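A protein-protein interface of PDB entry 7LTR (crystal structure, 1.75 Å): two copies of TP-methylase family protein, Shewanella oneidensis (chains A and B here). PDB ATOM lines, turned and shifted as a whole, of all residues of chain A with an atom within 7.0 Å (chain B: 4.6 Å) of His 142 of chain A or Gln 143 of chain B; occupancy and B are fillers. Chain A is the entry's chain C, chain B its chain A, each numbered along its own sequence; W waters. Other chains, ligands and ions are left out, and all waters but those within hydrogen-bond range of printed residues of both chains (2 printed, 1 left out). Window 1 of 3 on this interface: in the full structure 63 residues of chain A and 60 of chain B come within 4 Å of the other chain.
A ring nitrogen (NE2) of His 142 of chain B sits at hydrogen-bond distance from the side-chain carboxylate (OE1) of Glu 126 of chain A, 2.9 Å away. O of His 142 of chain B sits at hydrogen-bond distance from N of Ser 144 of chain A (2.8 Å). OE1 of Gln 143 of chain B sits close to OE1 of Gln 143 of chain A (3.1 Å). O of His 142 of chain A sits at hydrogen-bond distance from N of Ser 144 of chain B (2.8 Å).
The side-chain amide nitrogen (NE2) of Gln 143 of chain B sits at hydrogen-bond distance from the backbone carbonyl oxygen (O) of Asp 158 of chain B, 2.8 Å away. N of Phe 145 of chain B sits at hydrogen-bond distance from O of Leu 164 of chain B, at 3.0 Å. NE2 of Gln 143 of chain A lies close to N of Asp 158 of chain A (2.8 Å). The backbone NH (N) of Phe 145 of chain A is in hydrogen-bond range of the backbone carbonyl oxygen (O) of Leu 164 of chain A (3.0 Å). The side-chain carboxylate (OD1) of Asp 158 of chain A sits at hydrogen-bond distance from the side-chain hydroxyl (OG1) of Thr 160 of chain A (2.6 Å). The backbone carbonyl oxygen (O) of Asp 158 of chain A lies within hydrogen-bond range of the side-chain hydroxyl (OG1) of Thr 161 of chain A (2.6 Å).
Among the printed residues, merely in contact across the chains: His 142 of chain A with Gln 143 of chain B, Gly 141 of chain A with Ser 144 of chain B, His 142 of chain A with His 142 of chain B, Phe 145 of chain A with Asp 158 of chain B, Thr 161 of chain A with Phe 145 of chain B, Phe 145 of chain A with Thr 161 of chain B, Gln 143 of chain A with His 142 of chain B, Asp 158 of chain A with Phe 145 of chain B and Gly 141 of chain A with Phe 145 of chain B.
His 142 of chain A touches three residues of chain B. Of the printed residues of chain A, His 142 of chain B touches Glu 126 (2.9 Å), His 142 (3.3 Å), Gln 143 (3.6 Å) and Ser 144 (2.8 Å). Of chain A, only His 142 and Gln 143 come within 4 Å of Gln 143 of chain B. Of the printed residues of chain A, Ser 144 of chain B touches Gly 141 and His 142. The nearest residue of chain A that does not touch Gln 143 of chain B is Ser 144 of chain A (4.9 Å).
Of the 20 printed residues of chain A, 8 touch a printed residue of chain B. Printed residues of chain A that touch a printed residue of chain B: Glu 126, Gly 141, His 142, Gln 143, Ser 144, Phe 145, Asp 158 and Thr 161. Of the 10 printed residues of chain B, 6 touch a printed residue of chain A. Among the printed residues, no Asp or Glu carboxylate lies within 4 Å of a Lys or Arg side-chain nitrogen of the other chain.
His 142 of chain A touches Gln 143 of chain B, and with the chains exchanged Gln 143 of chain A touches His 142 of chain B. Gln 143 of chain A touches its own counterpart, Gln 143 of chain B. Phe 145 of chain A touches Asp 158 of chain B, and with the chains exchanged Asp 158 of chain A touches Phe 145 of chain B. Phe 145 of chain A touches Thr 161 of chain B, and with the chains exchanged Thr 161 of chain A touches Phe 145 of chain B. 9 positions are printed for both chains. Of the 13 pairs that touch across the chains among the printed residues, 10 have their exchanged pair printed and touching as well.
Water W2 lies within hydrogen-bond range of O of Val 156 of chain A (2.7 Å), OE1 of Gln 143 of chain A (2.9 Å) and N of Asp 158 of chain B (3.4 Å). Water W1 bridges ND1 of His 142 of chain A (3.0 Å) and OG of Ser 144 of chain B (3.3 Å).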
ATOM      1  N   GLU A 126      -0.155  13.843 -10.682  1.00  0.00           N
ATOM      2  CA  GLU A 126       1.299  13.888 -10.368  1.00  0.00           C
ATOM      3  C   GLU A 126       1.777  15.343 -10.394  1.00  0.00           C
ATOM      4  O   GLU A 126       2.529  15.743  -9.477  1.00  0.00           O
ATOM      5  CB  GLU A 126       2.091  13.026 -11.351  1.00  0.00           C
ATOM      6  CG  GLU A 126       3.556  12.874 -10.981  1.00  0.00           C
ATOM      7  CD  GLU A 126       4.300  11.876 -11.850  1.00  0.00           C
ATOM      8  OE1 GLU A 126       3.870  10.708 -11.898  1.00  0.00           O
ATOM      9  OE2 GLU A 126       5.287  12.273 -12.492  1.00  0.00           O
ATOM     10  N   TRP A 130       3.315  17.552  -6.871  1.00  0.00           N
ATOM     11  CA  TRP A 130       4.590  18.310  -6.740  1.00  0.00           C
ATOM     12  C   TRP A 130       4.289  19.723  -6.230  1.00  0.00           C
ATOM     13  O   TRP A 130       5.030  20.207  -5.357  1.00  0.00           O
ATOM     14  CB  TRP A 130       5.381  18.372  -8.053  1.00  0.00           C
ATOM     15  CG  TRP A 130       5.692  17.054  -8.695  1.00  0.00           C
ATOM     16  CD1 TRP A 130       5.512  16.740 -10.009  1.00  0.00           C
ATOM     17  CD2 TRP A 130       6.256  15.881  -8.077  1.00  0.00           C
ATOM     18  NE1 TRP A 130       5.918  15.457 -10.254  1.00  0.00           N
ATOM     19  CE2 TRP A 130       6.372  14.903  -9.088  1.00  0.00           C
ATOM     20  CE3 TRP A 130       6.663  15.554  -6.779  1.00  0.00           C
ATOM     21  CZ2 TRP A 130       6.878  13.628  -8.838  1.00  0.00           C
ATOM     22  CZ3 TRP A 130       7.166  14.294  -6.534  1.00  0.00           C
ATOM     23  CH2 TRP A 130       7.267  13.345  -7.551  1.00  0.00           C
ATOM     24  N   ASP A 136      10.061  18.671  -5.559  1.00  0.00           N
ATOM     25  CA  ASP A 136      10.583  18.581  -6.945  1.00  0.00           C
ATOM     26  C   ASP A 136      10.999  17.137  -7.207  1.00  0.00           C
ATOM     27  O   ASP A 136      11.823  16.591  -6.479  1.00  0.00           O
ATOM     28  CB  ASP A 136      11.743  19.557  -7.146  1.00  0.00           C
ATOM     29  CG  ASP A 136      12.259  19.607  -8.572  1.00  0.00           C
ATOM     30  OD1 ASP A 136      11.962  18.667  -9.334  1.00  0.00           O
ATOM     31  OD2 ASP A 136      12.948  20.590  -8.910  1.00  0.00           O
ATOM     32  N   PRO A 137      10.457  16.472  -8.253  1.00  0.00           N
ATOM     33  CA  PRO A 137      10.873  15.108  -8.582  1.00  0.00           C
ATOM     34  C   PRO A 137      12.387  15.033  -8.821  1.00  0.00           C
ATOM     35  O   PRO A 137      12.970  13.980  -8.613  1.00  0.00           O
ATOM     36  CB  PRO A 137      10.097  14.776  -9.866  1.00  0.00           C
ATOM     37  CG  PRO A 137       9.677  16.129 -10.411  1.00  0.00           C
ATOM     38  CD  PRO A 137       9.445  16.988  -9.185  1.00  0.00           C
ATOM     39  N   GLY A 138      12.983  16.153  -9.242  1.00  0.00           N
ATOM     40  CA  GLY A 138      14.408  16.237  -9.613  1.00  0.00           C
ATOM     41  C   GLY A 138      15.315  16.361  -8.399  1.00  0.00           C
ATOM     42  O   GLY A 138      16.532  16.162  -8.558  1.00  0.00           O
ATOM     43  N   ASN A 139      14.755  16.684  -7.229  1.00  0.00           N
ATOM     44  CA  ASN A 139      15.539  17.000  -6.004  1.00  0.00           C
ATOM     45  C   ASN A 139      16.452  15.819  -5.661  1.00  0.00           C
ATOM     46  O   ASN A 139      17.655  16.050  -5.446  1.00  0.00           O
ATOM     47  CB  ASN A 139      14.663  17.343  -4.800  1.00  0.00           C
ATOM     48  CG  ASN A 139      15.488  17.836  -3.630  1.00  0.00           C
ATOM     49  OD1 ASN A 139      15.675  17.121  -2.646  1.00  0.00           O
ATOM     50  ND2 ASN A 139      16.020  19.041  -3.746  1.00  0.00           N
ATOM     51  N   SER A 140      15.898  14.604  -5.589  1.00  0.00           N
ATOM     52  CA  SER A 140      16.663  13.352  -5.348  1.00  0.00           C
ATOM     53  C   SER A 140      16.156  12.239  -6.270  1.00  0.00           C
ATOM     54  O   SER A 140      16.454  11.064  -5.996  1.00  0.00           O
ATOM     55  CB  SER A 140      16.609  12.943  -3.899  1.00  0.00           C
ATOM     56  OG  SER A 140      15.281  12.642  -3.497  1.00  0.00           O
ATOM     57  N   GLY A 141      15.447  12.604  -7.340  1.00  0.00           N
ATOM     58  CA  GLY A 141      14.905  11.647  -8.322  1.00  0.00           C
ATOM     59  C   GLY A 141      13.510  11.193  -7.938  1.00  0.00           C
ATOM     60  O   GLY A 141      13.070  11.491  -6.804  1.00  0.00           O
ATOM     61  N   HIS A 142      12.835  10.481  -8.841  1.00  0.00           N
ATOM     62  CA  HIS A 142      11.404  10.112  -8.702  1.00  0.00           C
ATOM     63  C   HIS A 142      11.154   8.756  -9.360  1.00  0.00           C
ATOM     64  O   HIS A 142      11.629   8.542 -10.482  1.00  0.00           O
ATOM     65  CB  HIS A 142      10.538  11.241  -9.278  1.00  0.00           C
ATOM     66  CG  HIS A 142       9.178  10.819  -9.719  1.00  0.00           C
ATOM     67  ND1 HIS A 142       8.671  11.163 -10.958  1.00  0.00           N
ATOM     68  CD2 HIS A 142       8.218  10.099  -9.100  1.00  0.00           C
ATOM     69  CE1 HIS A 142       7.454  10.673 -11.082  1.00  0.00           C
ATOM     70  NE2 HIS A 142       7.153  10.013  -9.956  1.00  0.00           N
ATOM     71  N   GLN A 143      10.439   7.874  -8.665  1.00  0.00           N
ATOM     72  CA  GLN A 143       9.936   6.596  -9.230  1.00  0.00           C
ATOM     73  C   GLN A 143       8.432   6.522  -8.956  1.00  0.00           C
ATOM     74  O   GLN A 143       8.034   6.727  -7.792  1.00  0.00           O
ATOM     75  CB  GLN A 143      10.690   5.403  -8.639  1.00  0.00           C
ATOM     76  CG  GLN A 143      12.165   5.368  -9.016  1.00  0.00           C
ATOM     77  CD  GLN A 143      12.842   4.104  -8.544  1.00  0.00           C
ATOM     78  OE1 GLN A 143      13.538   3.426  -9.298  1.00  0.00           O
ATOM     79  NE2 GLN A 143      12.628   3.773  -7.282  1.00  0.00           N
ATOM     80  N   SER A 144       7.641   6.282 -10.004  1.00  0.00           N
ATOM     81  CA  SER A 144       6.171   6.075  -9.939  1.00  0.00           C
ATOM     82  C   SER A 144       5.840   4.658 -10.413  1.00  0.00           C
ATOM     83  O   SER A 144       6.269   4.286 -11.519  1.00  0.00           O
ATOM     84  CB  SER A 144       5.430   7.105 -10.757  1.00  0.00           C
ATOM     85  OG  SER A 144       5.139   8.260  -9.985  1.00  0.00           O
ATOM     86  N   PHE A 145       5.110   3.901  -9.596  1.00  0.00           N
ATOM     87  CA  PHE A 145       4.521   2.592  -9.971  1.00  0.00           C
ATOM     88  C   PHE A 145       3.042   2.593  -9.588  1.00  0.00           C
ATOM     89  O   PHE A 145       2.661   3.273  -8.617  1.00  0.00           O
ATOM     90  CB  PHE A 145       5.232   1.427  -9.277  1.00  0.00           C
ATOM     91  CG  PHE A 145       6.724   1.380  -9.478  1.00  0.00           C
ATOM     92  CD1 PHE A 145       7.273   0.774 -10.596  1.00  0.00           C
ATOM     93  CD2 PHE A 145       7.578   1.938  -8.541  1.00  0.00           C
ATOM     94  CE1 PHE A 145       8.646   0.733 -10.776  1.00  0.00           C
ATOM     95  CE2 PHE A 145       8.951   1.896  -8.722  1.00  0.00           C
ATOM     96  CZ  PHE A 145       9.481   1.295  -9.839  1.00  0.00           C
ATOM     97  N   VAL A 156      12.185  -3.148  -7.302  1.00  0.00           N
ATOM     98  CA  VAL A 156      12.974  -2.719  -6.112  1.00  0.00           C
ATOM     99  C   VAL A 156      13.220  -1.219  -6.226  1.00  0.00           C
ATOM    100  O   VAL A 156      13.932  -0.770  -7.121  1.00  0.00           O
ATOM    101  CB  VAL A 156      14.292  -3.504  -5.984  1.00  0.00           C
ATOM    102  CG1 VAL A 156      15.106  -3.032  -4.790  1.00  0.00           C
ATOM    103  CG2 VAL A 156      14.041  -5.003  -5.908  1.00  0.00           C
ATOM    104  N   ASP A 158      14.545   2.705  -5.569  1.00  0.00           N
ATOM    105  CA  ASP A 158      15.735   3.477  -5.131  1.00  0.00           C
ATOM    106  C   ASP A 158      15.299   4.350  -3.960  1.00  0.00           C
ATOM    107  O   ASP A 158      14.580   5.329  -4.148  1.00  0.00           O
ATOM    108  CB  ASP A 158      16.314   4.278  -6.299  1.00  0.00           C
ATOM    109  CG  ASP A 158      17.519   5.126  -5.931  1.00  0.00           C
ATOM    110  OD1 ASP A 158      17.812   5.237  -4.721  1.00  0.00           O
ATOM    111  OD2 ASP A 158      18.141   5.683  -6.859  1.00  0.00           O
ATOM    112  N   THR A 160      16.528   6.592  -2.186  1.00  0.00           N
ATOM    113  CA  THR A 160      16.987   8.006  -2.184  1.00  0.00           C
ATOM    114  C   THR A 160      15.955   8.878  -2.910  1.00  0.00           C
ATOM    115  O   THR A 160      16.015  10.110  -2.745  1.00  0.00           O
ATOM    116  CB  THR A 160      18.373   8.158  -2.821  1.00  0.00           C
ATOM    117  OG1 THR A 160      18.282   7.761  -4.189  1.00  0.00           O
ATOM    118  CG2 THR A 160      19.431   7.343  -2.112  1.00  0.00           C
ATOM    119  N   THR A 161      15.048   8.264  -3.677  1.00  0.00           N
ATOM    120  CA  THR A 161      14.058   8.977  -4.527  1.00  0.00           C
ATOM    121  C   THR A 161      12.778   9.254  -3.738  1.00  0.00           C
ATOM    122  O   THR A 161      12.589   8.664  -2.657  1.00  0.00           O
ATOM    123  CB  THR A 161      13.699   8.191  -5.795  1.00  0.00           C
ATOM    124  OG1 THR A 161      13.011   6.996  -5.417  1.00  0.00           O
ATOM    125  CG2 THR A 161      14.908   7.855  -6.640  1.00  0.00           C
ATOM    126  N   HIS A 162      11.932  10.134  -4.272  1.00  0.00           N
ATOM    127  CA  HIS A 162      10.493  10.200  -3.921  1.00  0.00           C
ATOM    128  C   HIS A 162       9.792   9.085  -4.698  1.00  0.00           C
ATOM    129  O   HIS A 162       9.846   9.112  -5.941  1.00  0.00           O
ATOM    130  CB  HIS A 162       9.925  11.596  -4.188  1.00  0.00           C
ATOM    131  CG  HIS A 162      10.224  12.558  -3.090  1.00  0.00           C
ATOM    132  ND1 HIS A 162      11.310  13.406  -3.130  1.00  0.00           N
ATOM    133  CD2 HIS A 162       9.591  12.799  -1.922  1.00  0.00           C
ATOM    134  CE1 HIS A 162      11.331  14.136  -2.034  1.00  0.00           C
ATOM    135  NE2 HIS A 162      10.290  13.780  -1.274  1.00  0.00           N
ATOM    136  N   LEU A 163       9.231   8.117  -3.973  1.00  0.00           N
ATOM    137  CA  LEU A 163       8.536   6.933  -4.537  1.00  0.00           C
ATOM    138  C   LEU A 163       7.029   7.174  -4.433  1.00  0.00           C
ATOM    139  O   LEU A 163       6.548   7.459  -3.314  1.00  0.00           O
ATOM    140  CB  LEU A 163       8.969   5.687  -3.760  1.00  0.00           C
ATOM    141  CG  LEU A 163       8.209   4.399  -4.077  1.00  0.00           C
ATOM    142  CD1 LEU A 163       8.443   3.965  -5.513  1.00  0.00           C
ATOM    143  CD2 LEU A 163       8.607   3.292  -3.114  1.00  0.00           C
ATOM    144  N   LEU A 164       6.331   7.115  -5.567  1.00  0.00           N
ATOM    145  CA  LEU A 164       4.857   7.277  -5.644  1.00  0.00           C
ATOM    146  C   LEU A 164       4.233   5.930  -6.012  1.00  0.00           C
ATOM    147  O   LEU A 164       4.649   5.343  -7.030  1.00  0.00           O
ATOM    148  CB  LEU A 164       4.509   8.340  -6.690  1.00  0.00           C
ATOM    149  CG  LEU A 164       4.969   9.763  -6.381  1.00  0.00           C
ATOM    150  CD1 LEU A 164       4.533  10.712  -7.487  1.00  0.00           C
ATOM    151  CD2 LEU A 164       4.436  10.233  -5.037  1.00  0.00           C
ATOM    152  N   TRP A 166       0.606   4.586  -7.058  1.00  0.00           N
ATOM    153  CA  TRP A 166      -0.692   5.068  -7.595  1.00  0.00           C
ATOM    154  C   TRP A 166      -1.780   4.021  -7.352  1.00  0.00           C
ATOM    155  O   TRP A 166      -1.444   2.828  -7.254  1.00  0.00           O
ATOM    156  CB  TRP A 166      -0.533   5.414  -9.075  1.00  0.00           C
ATOM    157  CG  TRP A 166       0.373   6.588  -9.256  1.00  0.00           C
ATOM    158  CD1 TRP A 166       1.714   6.572  -9.510  1.00  0.00           C
ATOM    159  CD2 TRP A 166       0.005   7.967  -9.106  1.00  0.00           C
ATOM    160  NE1 TRP A 166       2.198   7.851  -9.565  1.00  0.00           N
ATOM    161  CE2 TRP A 166       1.173   8.728  -9.322  1.00  0.00           C
ATOM    162  CE3 TRP A 166      -1.197   8.628  -8.837  1.00  0.00           C
ATOM    163  CZ2 TRP A 166       1.167  10.120  -9.271  1.00  0.00           C
ATOM    164  CZ3 TRP A 166      -1.201  10.004  -8.785  1.00  0.00           C
ATOM    165  CH2 TRP A 166      -0.034  10.737  -9.000  1.00  0.00           C
ATOM    166  N   HIS B 142       7.087   4.796 -14.283  1.00  0.00           N
ATOM    167  CA  HIS B 142       8.116   5.687 -14.879  1.00  0.00           C
ATOM    168  C   HIS B 142       9.053   6.189 -13.777  1.00  0.00           C
ATOM    169  O   HIS B 142       8.663   6.162 -12.595  1.00  0.00           O
ATOM    170  CB  HIS B 142       7.447   6.826 -15.664  1.00  0.00           C
ATOM    171  CG  HIS B 142       6.615   7.741 -14.830  1.00  0.00           C
ATOM    172  ND1 HIS B 142       5.345   7.405 -14.404  1.00  0.00           N
ATOM    173  CD2 HIS B 142       6.859   8.982 -14.353  1.00  0.00           C
ATOM    174  CE1 HIS B 142       4.845   8.397 -13.692  1.00  0.00           C
ATOM    175  NE2 HIS B 142       5.756   9.374 -13.644  1.00  0.00           N
ATOM    176  N   GLN B 143      10.255   6.608 -14.159  1.00  0.00           N
ATOM    177  CA  GLN B 143      11.263   7.154 -13.218  1.00  0.00           C
ATOM    178  C   GLN B 143      11.968   8.328 -13.887  1.00  0.00           C
ATOM    179  O   GLN B 143      12.106   8.306 -15.119  1.00  0.00           O
ATOM    180  CB  GLN B 143      12.312   6.110 -12.845  1.00  0.00           C
ATOM    181  CG  GLN B 143      11.856   4.674 -13.024  1.00  0.00           C
ATOM    182  CD  GLN B 143      13.050   3.774 -13.221  1.00  0.00           C
ATOM    183  OE1 GLN B 143      13.937   3.698 -12.373  1.00  0.00           O
ATOM    184  NE2 GLN B 143      13.088   3.095 -14.357  1.00  0.00           N
ATOM    185  N   SER B 144      12.397   9.300 -13.085  1.00  0.00           N
ATOM    186  CA  SER B 144      13.135  10.501 -13.545  1.00  0.00           C
ATOM    187  C   SER B 144      14.320  10.764 -12.617  1.00  0.00           C
ATOM    188  O   SER B 144      14.137  10.713 -11.384  1.00  0.00           O
ATOM    189  CB  SER B 144      12.223  11.691 -13.618  1.00  0.00           C
ATOM    190  OG  SER B 144      11.347  11.579 -14.727  1.00  0.00           O
ATOM    191  N   PHE B 145      15.485  11.037 -13.205  1.00  0.00           N
ATOM    192  CA  PHE B 145      16.688  11.545 -12.502  1.00  0.00           C
ATOM    193  C   PHE B 145      17.314  12.665 -13.333  1.00  0.00           C
ATOM    194  O   PHE B 145      17.294  12.578 -14.574  1.00  0.00           O
ATOM    195  CB  PHE B 145      17.727  10.441 -12.295  1.00  0.00           C
ATOM    196  CG  PHE B 145      17.226   9.199 -11.606  1.00  0.00           C
ATOM    197  CD1 PHE B 145      17.208   9.112 -10.224  1.00  0.00           C
ATOM    198  CD2 PHE B 145      16.792   8.109 -12.342  1.00  0.00           C
ATOM    199  CE1 PHE B 145      16.753   7.966  -9.592  1.00  0.00           C
ATOM    200  CE2 PHE B 145      16.342   6.961 -11.708  1.00  0.00           C
ATOM    201  CZ  PHE B 145      16.322   6.893 -10.336  1.00  0.00           C
ATOM    202  N   PRO B 157      18.338   2.563 -11.229  1.00  0.00           N
ATOM    203  CA  PRO B 157      17.093   2.596 -11.983  1.00  0.00           C
ATOM    204  C   PRO B 157      16.475   1.193 -12.003  1.00  0.00           C
ATOM    205  O   PRO B 157      17.190   0.231 -11.783  1.00  0.00           O
ATOM    206  CB  PRO B 157      17.554   3.015 -13.382  1.00  0.00           C
ATOM    207  CG  PRO B 157      18.920   2.371 -13.505  1.00  0.00           C
ATOM    208  CD  PRO B 157      19.511   2.411 -12.105  1.00  0.00           C
ATOM    209  N   ASP B 158      15.173   1.121 -12.262  1.00  0.00           N
ATOM    210  CA  ASP B 158      14.446  -0.151 -12.491  1.00  0.00           C
ATOM    211  C   ASP B 158      14.332  -0.332 -13.999  1.00  0.00           C
ATOM    212  O   ASP B 158      13.593   0.394 -14.659  1.00  0.00           O
ATOM    213  CB  ASP B 158      13.098  -0.130 -11.771  1.00  0.00           C
ATOM    214  CG  ASP B 158      12.256  -1.370 -12.012  1.00  0.00           C
ATOM    215  OD1 ASP B 158      12.628  -2.167 -12.898  1.00  0.00           O
ATOM    216  OD2 ASP B 158      11.239  -1.526 -11.307  1.00  0.00           O
ATOM    217  N   THR B 161      11.140  -0.466 -16.387  1.00  0.00           N
ATOM    218  CA  THR B 161      10.282   0.745 -16.324  1.00  0.00           C
ATOM    219  C   THR B 161      10.946   1.899 -17.084  1.00  0.00           C
ATOM    220  O   THR B 161      12.179   2.047 -16.968  1.00  0.00           O
ATOM    221  CB  THR B 161      10.016   1.122 -14.863  1.00  0.00           C
ATOM    222  OG1 THR B 161       9.412  -0.005 -14.226  1.00  0.00           O
ATOM    223  CG2 THR B 161       9.133   2.339 -14.715  1.00  0.00           C
ATOM    224  N   HIS B 162      10.153   2.687 -17.815  1.00  0.00           N
ATOM    225  CA  HIS B 162      10.615   3.874 -18.583  1.00  0.00           C
ATOM    226  C   HIS B 162      11.487   4.752 -17.684  1.00  0.00           C
ATOM    227  O   HIS B 162      11.047   5.082 -16.564  1.00  0.00           O
ATOM    228  CB  HIS B 162       9.431   4.661 -19.155  1.00  0.00           C
ATOM    229  CG  HIS B 162       8.758   3.980 -20.297  1.00  0.00           C
ATOM    230  ND1 HIS B 162       9.381   3.794 -21.514  1.00  0.00           N
ATOM    231  CD2 HIS B 162       7.523   3.449 -20.416  1.00  0.00           C
ATOM    232  CE1 HIS B 162       8.559   3.174 -22.335  1.00  0.00           C
ATOM    233  NE2 HIS B 162       7.414   2.947 -21.684  1.00  0.00           N
ATOM    234  N   LEU B 163      12.678   5.108 -18.168  1.00  0.00           N
ATOM    235  CA  LEU B 163      13.667   5.940 -17.436  1.00  0.00           C
ATOM    236  C   LEU B 163      13.888   7.244 -18.208  1.00  0.00           C
ATOM    237  O   LEU B 163      14.281   7.171 -19.384  1.00  0.00           O
ATOM    238  CB  LEU B 163      14.975   5.153 -17.299  1.00  0.00           C
ATOM    239  CG  LEU B 163      16.169   5.950 -16.776  1.00  0.00           C
ATOM    240  CD1 LEU B 163      15.934   6.398 -15.344  1.00  0.00           C
ATOM    241  CD2 LEU B 163      17.448   5.132 -16.874  1.00  0.00           C
ATOM    242  N   LEU B 164      13.636   8.386 -17.564  1.00  0.00           N
ATOM    243  CA  LEU B 164      13.956   9.732 -18.105  1.00  0.00           C
ATOM    244  C   LEU B 164      15.195  10.273 -17.392  1.00  0.00           C
ATOM    245  O   LEU B 164      15.182  10.315 -16.151  1.00  0.00           O
ATOM    246  CB  LEU B 164      12.778  10.683 -17.879  1.00  0.00           C
ATOM    247  CG  LEU B 164      11.512  10.399 -18.683  1.00  0.00           C
ATOM    248  CD1 LEU B 164      10.655  11.651 -18.769  1.00  0.00           C
ATOM    249  CD2 LEU B 164      11.849   9.887 -20.074  1.00  0.00           C
HETATM  250  O   HOH W   1       9.110  13.269 -13.050  1.00  0.00           O
HETATM  251  O   HOH W   2      15.055   1.018  -8.834  1.00  0.00           O
